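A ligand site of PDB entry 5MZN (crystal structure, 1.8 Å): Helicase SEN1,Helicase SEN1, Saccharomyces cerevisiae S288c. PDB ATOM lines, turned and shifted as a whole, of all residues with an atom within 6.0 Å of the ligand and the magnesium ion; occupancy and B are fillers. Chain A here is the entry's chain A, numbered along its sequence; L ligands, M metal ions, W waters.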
ATOM      1  N   LYS A 243       2.758  19.288   8.500  1.00  0.00           N
ATOM      2  CA  LYS A 243       2.351  18.175   9.373  1.00  0.00           C
ATOM      3  C   LYS A 243       3.281  16.984   9.166  1.00  0.00           C
ATOM      4  O   LYS A 243       2.880  15.898   8.758  1.00  0.00           O
ATOM      5  CB  LYS A 243       0.895  17.808   9.125  1.00  0.00           C
ATOM      6  CG  LYS A 243      -0.035  19.019   9.205  1.00  0.00           C
ATOM      7  CD  LYS A 243      -1.465  18.624   9.520  1.00  0.00           C
ATOM      8  CE  LYS A 243      -2.345  19.860   9.714  1.00  0.00           C
ATOM      9  NZ  LYS A 243      -2.491  20.624   8.455  1.00  0.00           N
ATOM     10  N   LEU A 244       4.545  17.231   9.430  1.00  0.00           N
ATOM     11  CA  LEU A 244       5.598  16.265   9.205  1.00  0.00           C
ATOM     12  C   LEU A 244       6.270  15.966  10.526  1.00  0.00           C
ATOM     13  O   LEU A 244       6.114  16.716  11.491  1.00  0.00           O
ATOM     14  CB  LEU A 244       6.642  16.811   8.253  1.00  0.00           C
ATOM     15  CG  LEU A 244       6.125  17.213   6.873  1.00  0.00           C
ATOM     16  CD1 LEU A 244       7.209  17.947   6.130  1.00  0.00           C
ATOM     17  CD2 LEU A 244       5.653  16.003   6.083  1.00  0.00           C
ATOM     18  N   ASN A 245       6.987  14.839  10.573  1.00  0.00           N
ATOM     19  CA  ASN A 245       7.851  14.603  11.702  1.00  0.00           C
ATOM     20  C   ASN A 245       9.188  15.284  11.455  1.00  0.00           C
ATOM     21  O   ASN A 245       9.494  15.760  10.353  1.00  0.00           O
ATOM     22  CB  ASN A 245       7.990  13.097  12.010  1.00  0.00           C
ATOM     23  CG  ASN A 245       8.680  12.323  10.914  1.00  0.00           C
ATOM     24  OD1 ASN A 245       9.757  12.710  10.429  1.00  0.00           O
ATOM     25  ND2 ASN A 245       8.091  11.164  10.551  1.00  0.00           N
ATOM     26  N   GLN A 248      11.427  14.122   8.522  1.00  0.00           N
ATOM     27  CA  GLN A 248      10.914  14.533   7.208  1.00  0.00           C
ATOM     28  C   GLN A 248      11.179  16.025   6.944  1.00  0.00           C
ATOM     29  O   GLN A 248      11.649  16.395   5.856  1.00  0.00           O
ATOM     30  CB  GLN A 248       9.430  14.239   7.128  1.00  0.00           C
ATOM     31  CG  GLN A 248       9.166  12.716   7.191  1.00  0.00           C
ATOM     32  CD  GLN A 248       7.707  12.408   7.445  1.00  0.00           C
ATOM     33  OE1 GLN A 248       6.985  13.198   8.063  1.00  0.00           O
ATOM     34  NE2 GLN A 248       7.264  11.256   6.979  1.00  0.00           N
ATOM     35  N   GLY A 266      14.156   6.245   3.016  1.00  0.00           N
ATOM     36  CA  GLY A 266      12.929   5.951   3.701  1.00  0.00           C
ATOM     37  C   GLY A 266      12.682   4.478   3.814  1.00  0.00           C
ATOM     38  O   GLY A 266      12.308   3.823   2.834  1.00  0.00           O
ATOM     39  N   PRO A 267      12.831   3.908   5.012  1.00  0.00           N
ATOM     40  CA  PRO A 267      12.430   2.525   5.209  1.00  0.00           C
ATOM     41  C   PRO A 267      10.940   2.352   4.949  1.00  0.00           C
ATOM     42  O   PRO A 267      10.196   3.332   4.743  1.00  0.00           O
ATOM     43  CB  PRO A 267      12.768   2.256   6.691  1.00  0.00           C
ATOM     44  CG  PRO A 267      13.835   3.287   7.005  1.00  0.00           C
ATOM     45  CD  PRO A 267      13.525   4.479   6.201  1.00  0.00           C
ATOM     46  N   PRO A 268      10.470   1.116   4.941  1.00  0.00           N
ATOM     47  CA  PRO A 268       9.033   0.859   4.696  1.00  0.00           C
ATOM     48  C   PRO A 268       8.134   1.695   5.581  1.00  0.00           C
ATOM     49  O   PRO A 268       8.289   1.729   6.797  1.00  0.00           O
ATOM     50  CB  PRO A 268       8.912  -0.638   5.007  1.00  0.00           C
ATOM     51  CG  PRO A 268      10.270  -1.201   4.649  1.00  0.00           C
ATOM     52  CD  PRO A 268      11.239  -0.124   5.128  1.00  0.00           C
ATOM     53  N   GLY A 269       7.185   2.398   4.954  1.00  0.00           N
ATOM     54  CA  GLY A 269       6.166   3.101   5.722  1.00  0.00           C
ATOM     55  C   GLY A 269       6.572   4.390   6.411  1.00  0.00           C
ATOM     56  O   GLY A 269       5.928   4.781   7.392  1.00  0.00           O
ATOM     57  N   THR A 270       7.650   5.037   5.979  1.00  0.00           N
ATOM     58  CA  THR A 270       8.172   6.201   6.668  1.00  0.00           C
ATOM     59  C   THR A 270       7.872   7.489   5.959  1.00  0.00           C
ATOM     60  O   THR A 270       8.383   8.532   6.376  1.00  0.00           O
ATOM     61  CB  THR A 270       9.689   6.078   6.875  1.00  0.00           C
ATOM     62  OG1 THR A 270      10.362   5.944   5.588  1.00  0.00           O
ATOM     63  CG2 THR A 270      10.000   4.889   7.730  1.00  0.00           C
ATOM     64  N   GLY A 271       7.071   7.469   4.879  1.00  0.00           N
ATOM     65  CA  GLY A 271       6.650   8.709   4.240  1.00  0.00           C
ATOM     66  C   GLY A 271       7.541   9.255   3.147  1.00  0.00           C
ATOM     67  O   GLY A 271       7.650  10.489   3.016  1.00  0.00           O
ATOM     68  N   LYS A 272       8.173   8.384   2.359  1.00  0.00           N
ATOM     69  CA  LYS A 272       8.951   8.827   1.203  1.00  0.00           C
ATOM     70  C   LYS A 272       8.086   9.700   0.300  1.00  0.00           C
ATOM     71  O   LYS A 272       8.455  10.835  -0.059  1.00  0.00           O
ATOM     72  CB  LYS A 272       9.474   7.617   0.420  1.00  0.00           C
ATOM     73  CG  LYS A 272      10.544   6.796   1.128  1.00  0.00           C
ATOM     74  CD  LYS A 272      10.941   5.514   0.361  1.00  0.00           C
ATOM     75  CE  LYS A 272       9.850   4.421   0.356  1.00  0.00           C
ATOM     76  NZ  LYS A 272       9.564   4.025   1.787  1.00  0.00           N
ATOM     77  N   THR A 273       6.937   9.180  -0.090  1.00  0.00           N
ATOM     78  CA  THR A 273       6.104   9.939  -1.031  1.00  0.00           C
ATOM     79  C   THR A 273       5.495  11.176  -0.377  1.00  0.00           C
ATOM     80  O   THR A 273       5.459  12.244  -0.997  1.00  0.00           O
ATOM     81  CB  THR A 273       5.056   8.997  -1.621  1.00  0.00           C
ATOM     82  OG1 THR A 273       5.745   7.906  -2.252  1.00  0.00           O
ATOM     83  CG2 THR A 273       4.199   9.731  -2.644  1.00  0.00           C
ATOM     84  N   LYS A 274       5.039  11.075   0.886  1.00  0.00           N
ATOM     85  CA  LYS A 274       4.565  12.244   1.607  1.00  0.00           C
ATOM     86  C   LYS A 274       5.633  13.335   1.657  1.00  0.00           C
ATOM     87  O   LYS A 274       5.327  14.513   1.485  1.00  0.00           O
ATOM     88  CB  LYS A 274       4.103  11.855   3.016  1.00  0.00           C
ATOM     89  CG  LYS A 274       3.532  13.037   3.851  1.00  0.00           C
ATOM     90  CD  LYS A 274       2.790  12.538   5.123  1.00  0.00           C
ATOM     91  CE  LYS A 274       1.417  13.202   5.304  1.00  0.00           C
ATOM     92  NZ  LYS A 274       0.349  12.187   5.505  1.00  0.00           N
ATOM     93  N   THR A 275       6.888  12.943   1.876  1.00  0.00           N
ATOM     94  CA  THR A 275       7.976  13.922   1.955  1.00  0.00           C
ATOM     95  C   THR A 275       8.198  14.588   0.599  1.00  0.00           C
ATOM     96  O   THR A 275       8.465  15.789   0.552  1.00  0.00           O
ATOM     97  CB  THR A 275       9.272  13.244   2.445  1.00  0.00           C
ATOM     98  OG1 THR A 275       9.106  12.746   3.779  1.00  0.00           O
ATOM     99  CG2 THR A 275      10.457  14.217   2.446  1.00  0.00           C
ATOM    100  N   GLU A 327       0.670   7.346  -8.338  1.00  0.00           N
ATOM    101  CA  GLU A 327       0.406   7.585  -6.915  1.00  0.00           C
ATOM    102  C   GLU A 327       0.718   9.025  -6.550  1.00  0.00           C
ATOM    103  O   GLU A 327      -0.064   9.691  -5.852  1.00  0.00           O
ATOM    104  CB  GLU A 327       1.218   6.635  -6.040  1.00  0.00           C
ATOM    105  CG  GLU A 327       0.827   6.862  -4.575  1.00  0.00           C
ATOM    106  CD  GLU A 327       1.559   6.007  -3.610  1.00  0.00           C
ATOM    107  OE1 GLU A 327       2.194   5.020  -4.043  1.00  0.00           O
ATOM    108  OE2 GLU A 327       1.475   6.336  -2.402  1.00  0.00           O
ATOM    109  N   ARG A 331      -1.991  11.862  -5.301  1.00  0.00           N
ATOM    110  CA  ARG A 331      -1.847  12.526  -4.018  1.00  0.00           C
ATOM    111  C   ARG A 331      -1.636  14.020  -4.160  1.00  0.00           C
ATOM    112  O   ARG A 331      -1.995  14.766  -3.237  1.00  0.00           O
ATOM    113  CB  ARG A 331      -0.692  11.855  -3.258  1.00  0.00           C
ATOM    114  CG  ARG A 331      -1.143  10.480  -2.772  1.00  0.00           C
ATOM    115  CD  ARG A 331      -0.042   9.680  -2.180  1.00  0.00           C
ATOM    116  NE  ARG A 331       0.375  10.185  -0.876  1.00  0.00           N
ATOM    117  CZ  ARG A 331       1.252   9.538  -0.116  1.00  0.00           C
ATOM    118  NH1 ARG A 331       1.690   8.360  -0.523  1.00  0.00           N
ATOM    119  NH2 ARG A 331       1.633   9.987   1.059  1.00  0.00           N
ATOM    120  N   ASP A 435      11.188   9.556  -6.899  1.00  0.00           N
ATOM    121  CA  ASP A 435      10.631   8.640  -5.902  1.00  0.00           C
ATOM    122  C   ASP A 435      11.028   7.209  -6.290  1.00  0.00           C
ATOM    123  O   ASP A 435      11.377   6.931  -7.434  1.00  0.00           O
ATOM    124  CB  ASP A 435       9.094   8.785  -5.821  1.00  0.00           C
ATOM    125  CG  ASP A 435       8.483   8.337  -4.512  1.00  0.00           C
ATOM    126  OD1 ASP A 435       9.178   7.772  -3.651  1.00  0.00           O
ATOM    127  OD2 ASP A 435       7.220   8.490  -4.360  1.00  0.00           O
ATOM    128  N   GLU A 436      10.929   6.279  -5.320  1.00  0.00           N
ATOM    129  CA  GLU A 436      11.292   4.868  -5.521  1.00  0.00           C
ATOM    130  C   GLU A 436      12.665   4.753  -6.207  1.00  0.00           C
ATOM    131  O   GLU A 436      12.856   3.944  -7.106  1.00  0.00           O
ATOM    132  CB  GLU A 436      10.207   4.151  -6.327  1.00  0.00           C
ATOM    133  CG  GLU A 436       8.826   4.281  -5.660  1.00  0.00           C
ATOM    134  CD  GLU A 436       8.677   3.351  -4.489  1.00  0.00           C
ATOM    135  OE1 GLU A 436       8.305   2.198  -4.761  1.00  0.00           O
ATOM    136  OE2 GLU A 436       8.903   3.736  -3.307  1.00  0.00           O
ATOM    137  N   LEU A 496      14.521   8.967   7.115  1.00  0.00           N
ATOM    138  CA  LEU A 496      13.163   9.118   7.610  1.00  0.00           C
ATOM    139  C   LEU A 496      12.945   8.052   8.679  1.00  0.00           C
ATOM    140  O   LEU A 496      13.034   6.865   8.369  1.00  0.00           O
ATOM    141  CB  LEU A 496      12.162   8.961   6.465  1.00  0.00           C
ATOM    142  CG  LEU A 496      12.377   9.884   5.256  1.00  0.00           C
ATOM    143  CD1 LEU A 496      11.221   9.732   4.281  1.00  0.00           C
ATOM    144  CD2 LEU A 496      12.600  11.366   5.653  1.00  0.00           C
ATOM    145  N   VAL A 498      10.500   7.375  11.303  1.00  0.00           N
ATOM    146  CA  VAL A 498       9.276   6.949  11.964  1.00  0.00           C
ATOM    147  C   VAL A 498       8.447   6.148  10.976  1.00  0.00           C
ATOM    148  O   VAL A 498       8.117   6.652   9.903  1.00  0.00           O
ATOM    149  CB  VAL A 498       8.428   8.127  12.499  1.00  0.00           C
ATOM    150  CG1 VAL A 498       7.218   7.582  13.246  1.00  0.00           C
ATOM    151  CG2 VAL A 498       9.238   9.112  13.384  1.00  0.00           C
ATOM    152  N   TYR A 500       4.938   4.041   9.973  1.00  0.00           N
ATOM    153  CA  TYR A 500       3.516   4.204  10.268  1.00  0.00           C
ATOM    154  C   TYR A 500       2.669   3.030   9.795  1.00  0.00           C
ATOM    155  O   TYR A 500       1.449   3.185   9.603  1.00  0.00           O
ATOM    156  CB  TYR A 500       2.977   5.504   9.653  1.00  0.00           C
ATOM    157  CG  TYR A 500       3.640   6.736  10.187  1.00  0.00           C
ATOM    158  CD1 TYR A 500       3.141   7.404  11.329  1.00  0.00           C
ATOM    159  CD2 TYR A 500       4.767   7.278   9.564  1.00  0.00           C
ATOM    160  CE1 TYR A 500       3.772   8.536  11.813  1.00  0.00           C
ATOM    161  CE2 TYR A 500       5.382   8.403  10.049  1.00  0.00           C
ATOM    162  CZ  TYR A 500       4.878   9.025  11.161  1.00  0.00           C
ATOM    163  OH  TYR A 500       5.533  10.133  11.638  1.00  0.00           O
ATOM    164  N   ARG A 501       3.246   1.860   9.633  1.00  0.00           N
ATOM    165  CA  ARG A 501       2.538   0.698   9.102  1.00  0.00           C
ATOM    166  C   ARG A 501       2.370  -0.455  10.071  1.00  0.00           C
ATOM    167  O   ARG A 501       1.323  -1.078  10.099  1.00  0.00           O
ATOM    168  CB  ARG A 501       3.298   0.135   7.883  1.00  0.00           C
ATOM    169  CG  ARG A 501       3.186   0.938   6.663  1.00  0.00           C
ATOM    170  CD  ARG A 501       4.192   0.380   5.633  1.00  0.00           C
ATOM    171  NE  ARG A 501       3.875  -0.984   5.187  1.00  0.00           N
ATOM    172  CZ  ARG A 501       4.567  -2.093   5.492  1.00  0.00           C
ATOM    173  NH1 ARG A 501       4.182  -3.261   4.995  1.00  0.00           N
ATOM    174  NH2 ARG A 501       5.632  -2.048   6.272  1.00  0.00           N
HETATM  175  P1  LIG L   1       6.132   5.580   1.612  1.00  0.00           P
HETATM  176  O1  LIG L   1       5.567   4.196   1.482  1.00  0.00           O
HETATM  177  O2  LIG L   1       6.179   6.395   0.375  1.00  0.00           O
HETATM  178  O3  LIG L   1       7.426   5.744   2.328  1.00  0.00           O
HETATM  179  P2  LIG L   1       3.799   7.238   2.331  1.00  0.00           P
HETATM  180  O4  LIG L   1       2.923   6.410   1.444  1.00  0.00           O
HETATM  181  O5  LIG L   1       4.039   8.686   2.048  1.00  0.00           O
HETATM  182  O6  LIG L   1       5.169   6.424   2.600  1.00  0.00           O
HETATM  183  O7  LIG L   1       3.142   7.164   3.818  1.00  0.00           O
HETATM  184  C1  LIG L   1       2.868   5.879   4.364  1.00  0.00           C
HETATM  185  C2  LIG L   1       1.994   6.017   5.609  1.00  0.00           C
HETATM  186  O8  LIG L   1       2.671   6.763   6.620  1.00  0.00           O
HETATM  187  C3  LIG L   1       0.729   6.808   5.294  1.00  0.00           C
HETATM  188  O9  LIG L   1      -0.354   6.176   5.976  1.00  0.00           O
HETATM  189  C4  LIG L   1       1.005   8.184   5.782  1.00  0.00           C
HETATM  190  O10 LIG L   1      -0.196   8.874   6.122  1.00  0.00           O
HETATM  191  C5  LIG L   1       1.837   7.858   7.001  1.00  0.00           C
HETATM  192  N1  LIG L   1       2.678   8.959   7.419  1.00  0.00           N
HETATM  193  C6  LIG L   1       3.814   9.336   6.854  1.00  0.00           C
HETATM  194  N2  LIG L   1       4.335  10.386   7.480  1.00  0.00           N
HETATM  195  C7  LIG L   1       3.503  10.653   8.505  1.00  0.00           C
HETATM  196  C8  LIG L   1       3.472  11.663   9.565  1.00  0.00           C
HETATM  197  N3  LIG L   1       4.485  12.529   9.612  1.00  0.00           N
HETATM  198  N4  LIG L   1       2.432  11.636  10.419  1.00  0.00           N
HETATM  199  C9  LIG L   1       1.448  10.715  10.294  1.00  0.00           C
HETATM  200  N5  LIG L   1       1.398   9.777   9.336  1.00  0.00           N
HETATM  201  C10 LIG L   1       2.411   9.722   8.449  1.00  0.00           C
HETATM  202 MG    MG M   1       5.838   5.892  -1.651  1.00  0.00          MG
HETATM  203  O   HOH W   1      -0.776   8.454   9.736  1.00  0.00           O
HETATM  204  O   HOH W   2       1.409   2.853   3.850  1.00  0.00           O
HETATM  205  O   HOH W   3       5.136   5.288  -3.639  1.00  0.00           O
HETATM  206  O   HOH W   4      -2.346   8.173   7.623  1.00  0.00           O
HETATM  207  O   HOH W   5       7.896   5.914  -2.227  1.00  0.00           O
HETATM  208  O   HOH W   6       7.218   2.199   2.055  1.00  0.00           O
HETATM  209  O   HOH W   7       3.859   2.825   3.032  1.00  0.00           O
HETATM  210  O   HOH W   8      -0.333   3.550   6.219  1.00  0.00           O
HETATM  211  O   HOH W   9       0.446   5.697   1.472  1.00  0.00           O
HETATM  212  O   HOH W  10       3.762   5.840  -1.201  1.00  0.00           O
HETATM  213  O   HOH W  11      -2.724   6.864   4.082  1.00  0.00           O
HETATM  214  O   HOH W  12       5.925   3.771  -1.155  1.00  0.00           O
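N of Thr 273 lies close to O2 of the ligand. The backbone NH (N) of Lys 272 is in hydrogen-bond range of an oxygen (O3) of the ligand (2.7 Å). An oxygen (O3) of the ligand is in salt-bridge range of the side-chain amino group (NZ) of Lys 272, at 2.8 Å. An oxygen (O5) of the ligand sits at hydrogen-bond distance from the backbone NH of Lys 274, at 2.8 Å. NZ of Lys 274 sits at hydrogen-bond distance from O10 of the ligand, 3.4 Å away. The guanidinium group (NH2) of Arg 331 lies within salt-bridge range of an oxygen (O5) of the ligand, at 2.9 Å. OE1 of Gln 248 sits at hydrogen-bond distance from N3 of the ligand. The backbone NH (N) of Gly 271 lies within hydrogen-bond range of an oxygen (O3) of the ligand, 3.1 Å away. N3 of the ligand sits close to OH of Tyr 500, 3.3 Å away.
The side-chain amino group of Lys 272 lies within hydrogen-bond range of the backbone carbonyl oxygen of Pro 267 (3.1 Å). The side-chain amino group (NZ) of Lys 272 sits at hydrogen-bond distance from the backbone carbonyl oxygen (O) of Gly 266 (2.9 Å). The guanidinium group (NH1) of Arg 331 is in salt-bridge range of the side-chain carboxylate (OE2) of Glu 327, 2.8 Å away. The backbone NH (N) of Gln 248 lies within hydrogen-bond range of the side-chain amide oxygen (OD1) of Asn 245 (2.9 Å). The side-chain amide nitrogen of Gln 248 lies within hydrogen-bond range of the backbone carbonyl oxygen of Thr 270 (3.0 Å). The side-chain hydroxyl of Tyr 500 lies within hydrogen-bond range of the side-chain amide nitrogen of Asn 245, 3.0 Å away. The backbone NH (N) of Tyr 500 lies within hydrogen-bond range of the backbone carbonyl oxygen (O) of Gly 269 (2.9 Å). O of Pro 267 is in hydrogen-bond range of OG1 of Thr 270.
Lys 243 touches the ligand (O to N3, 3.8 Å). Leu 244 touches the ligand. N of Asn 245 touches N3 of the ligand (3.5 Å). O of Gly 269 touches O8 of the ligand, 3.9 Å away. N of Thr 270 touches O3 of the ligand (3.7 Å). Hydrophobic or aromatic side chains within 4 Å of the ligand: Tyr 500. Within 4 Å of the ligand: Lys 243, Leu 244, Asn 245, Gln 248, Gly 269, Thr 270, Gly 271, Lys 272, Thr 273, Lys 274, Arg 331 and Tyr 500. The nearest printed residue that does not touch the ligand is Glu 327 (4.1 Å).
OD2 of Asp 435 touches the magnesium ion, 3.9998 Å away.
The magnesium ion is bound by OG1 of Thr 273, O2 of the ligand, water W10, water W5, water W12 and water W3.
Water W10 lies within hydrogen-bond range of OE2 of Glu 327 (2.6 Å), O4 of the ligand (2.8 Å) and NH1 of Arg 331 (3.3 Å). Water W5 bridges OE2 of Glu 436 and OD1 of Asp 435. Water W6 lies within hydrogen-bond range of an oxygen (O1) of the ligand, the backbone NH (N) of Gly 269 and the side-chain amino group (NZ) of Lys 272.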
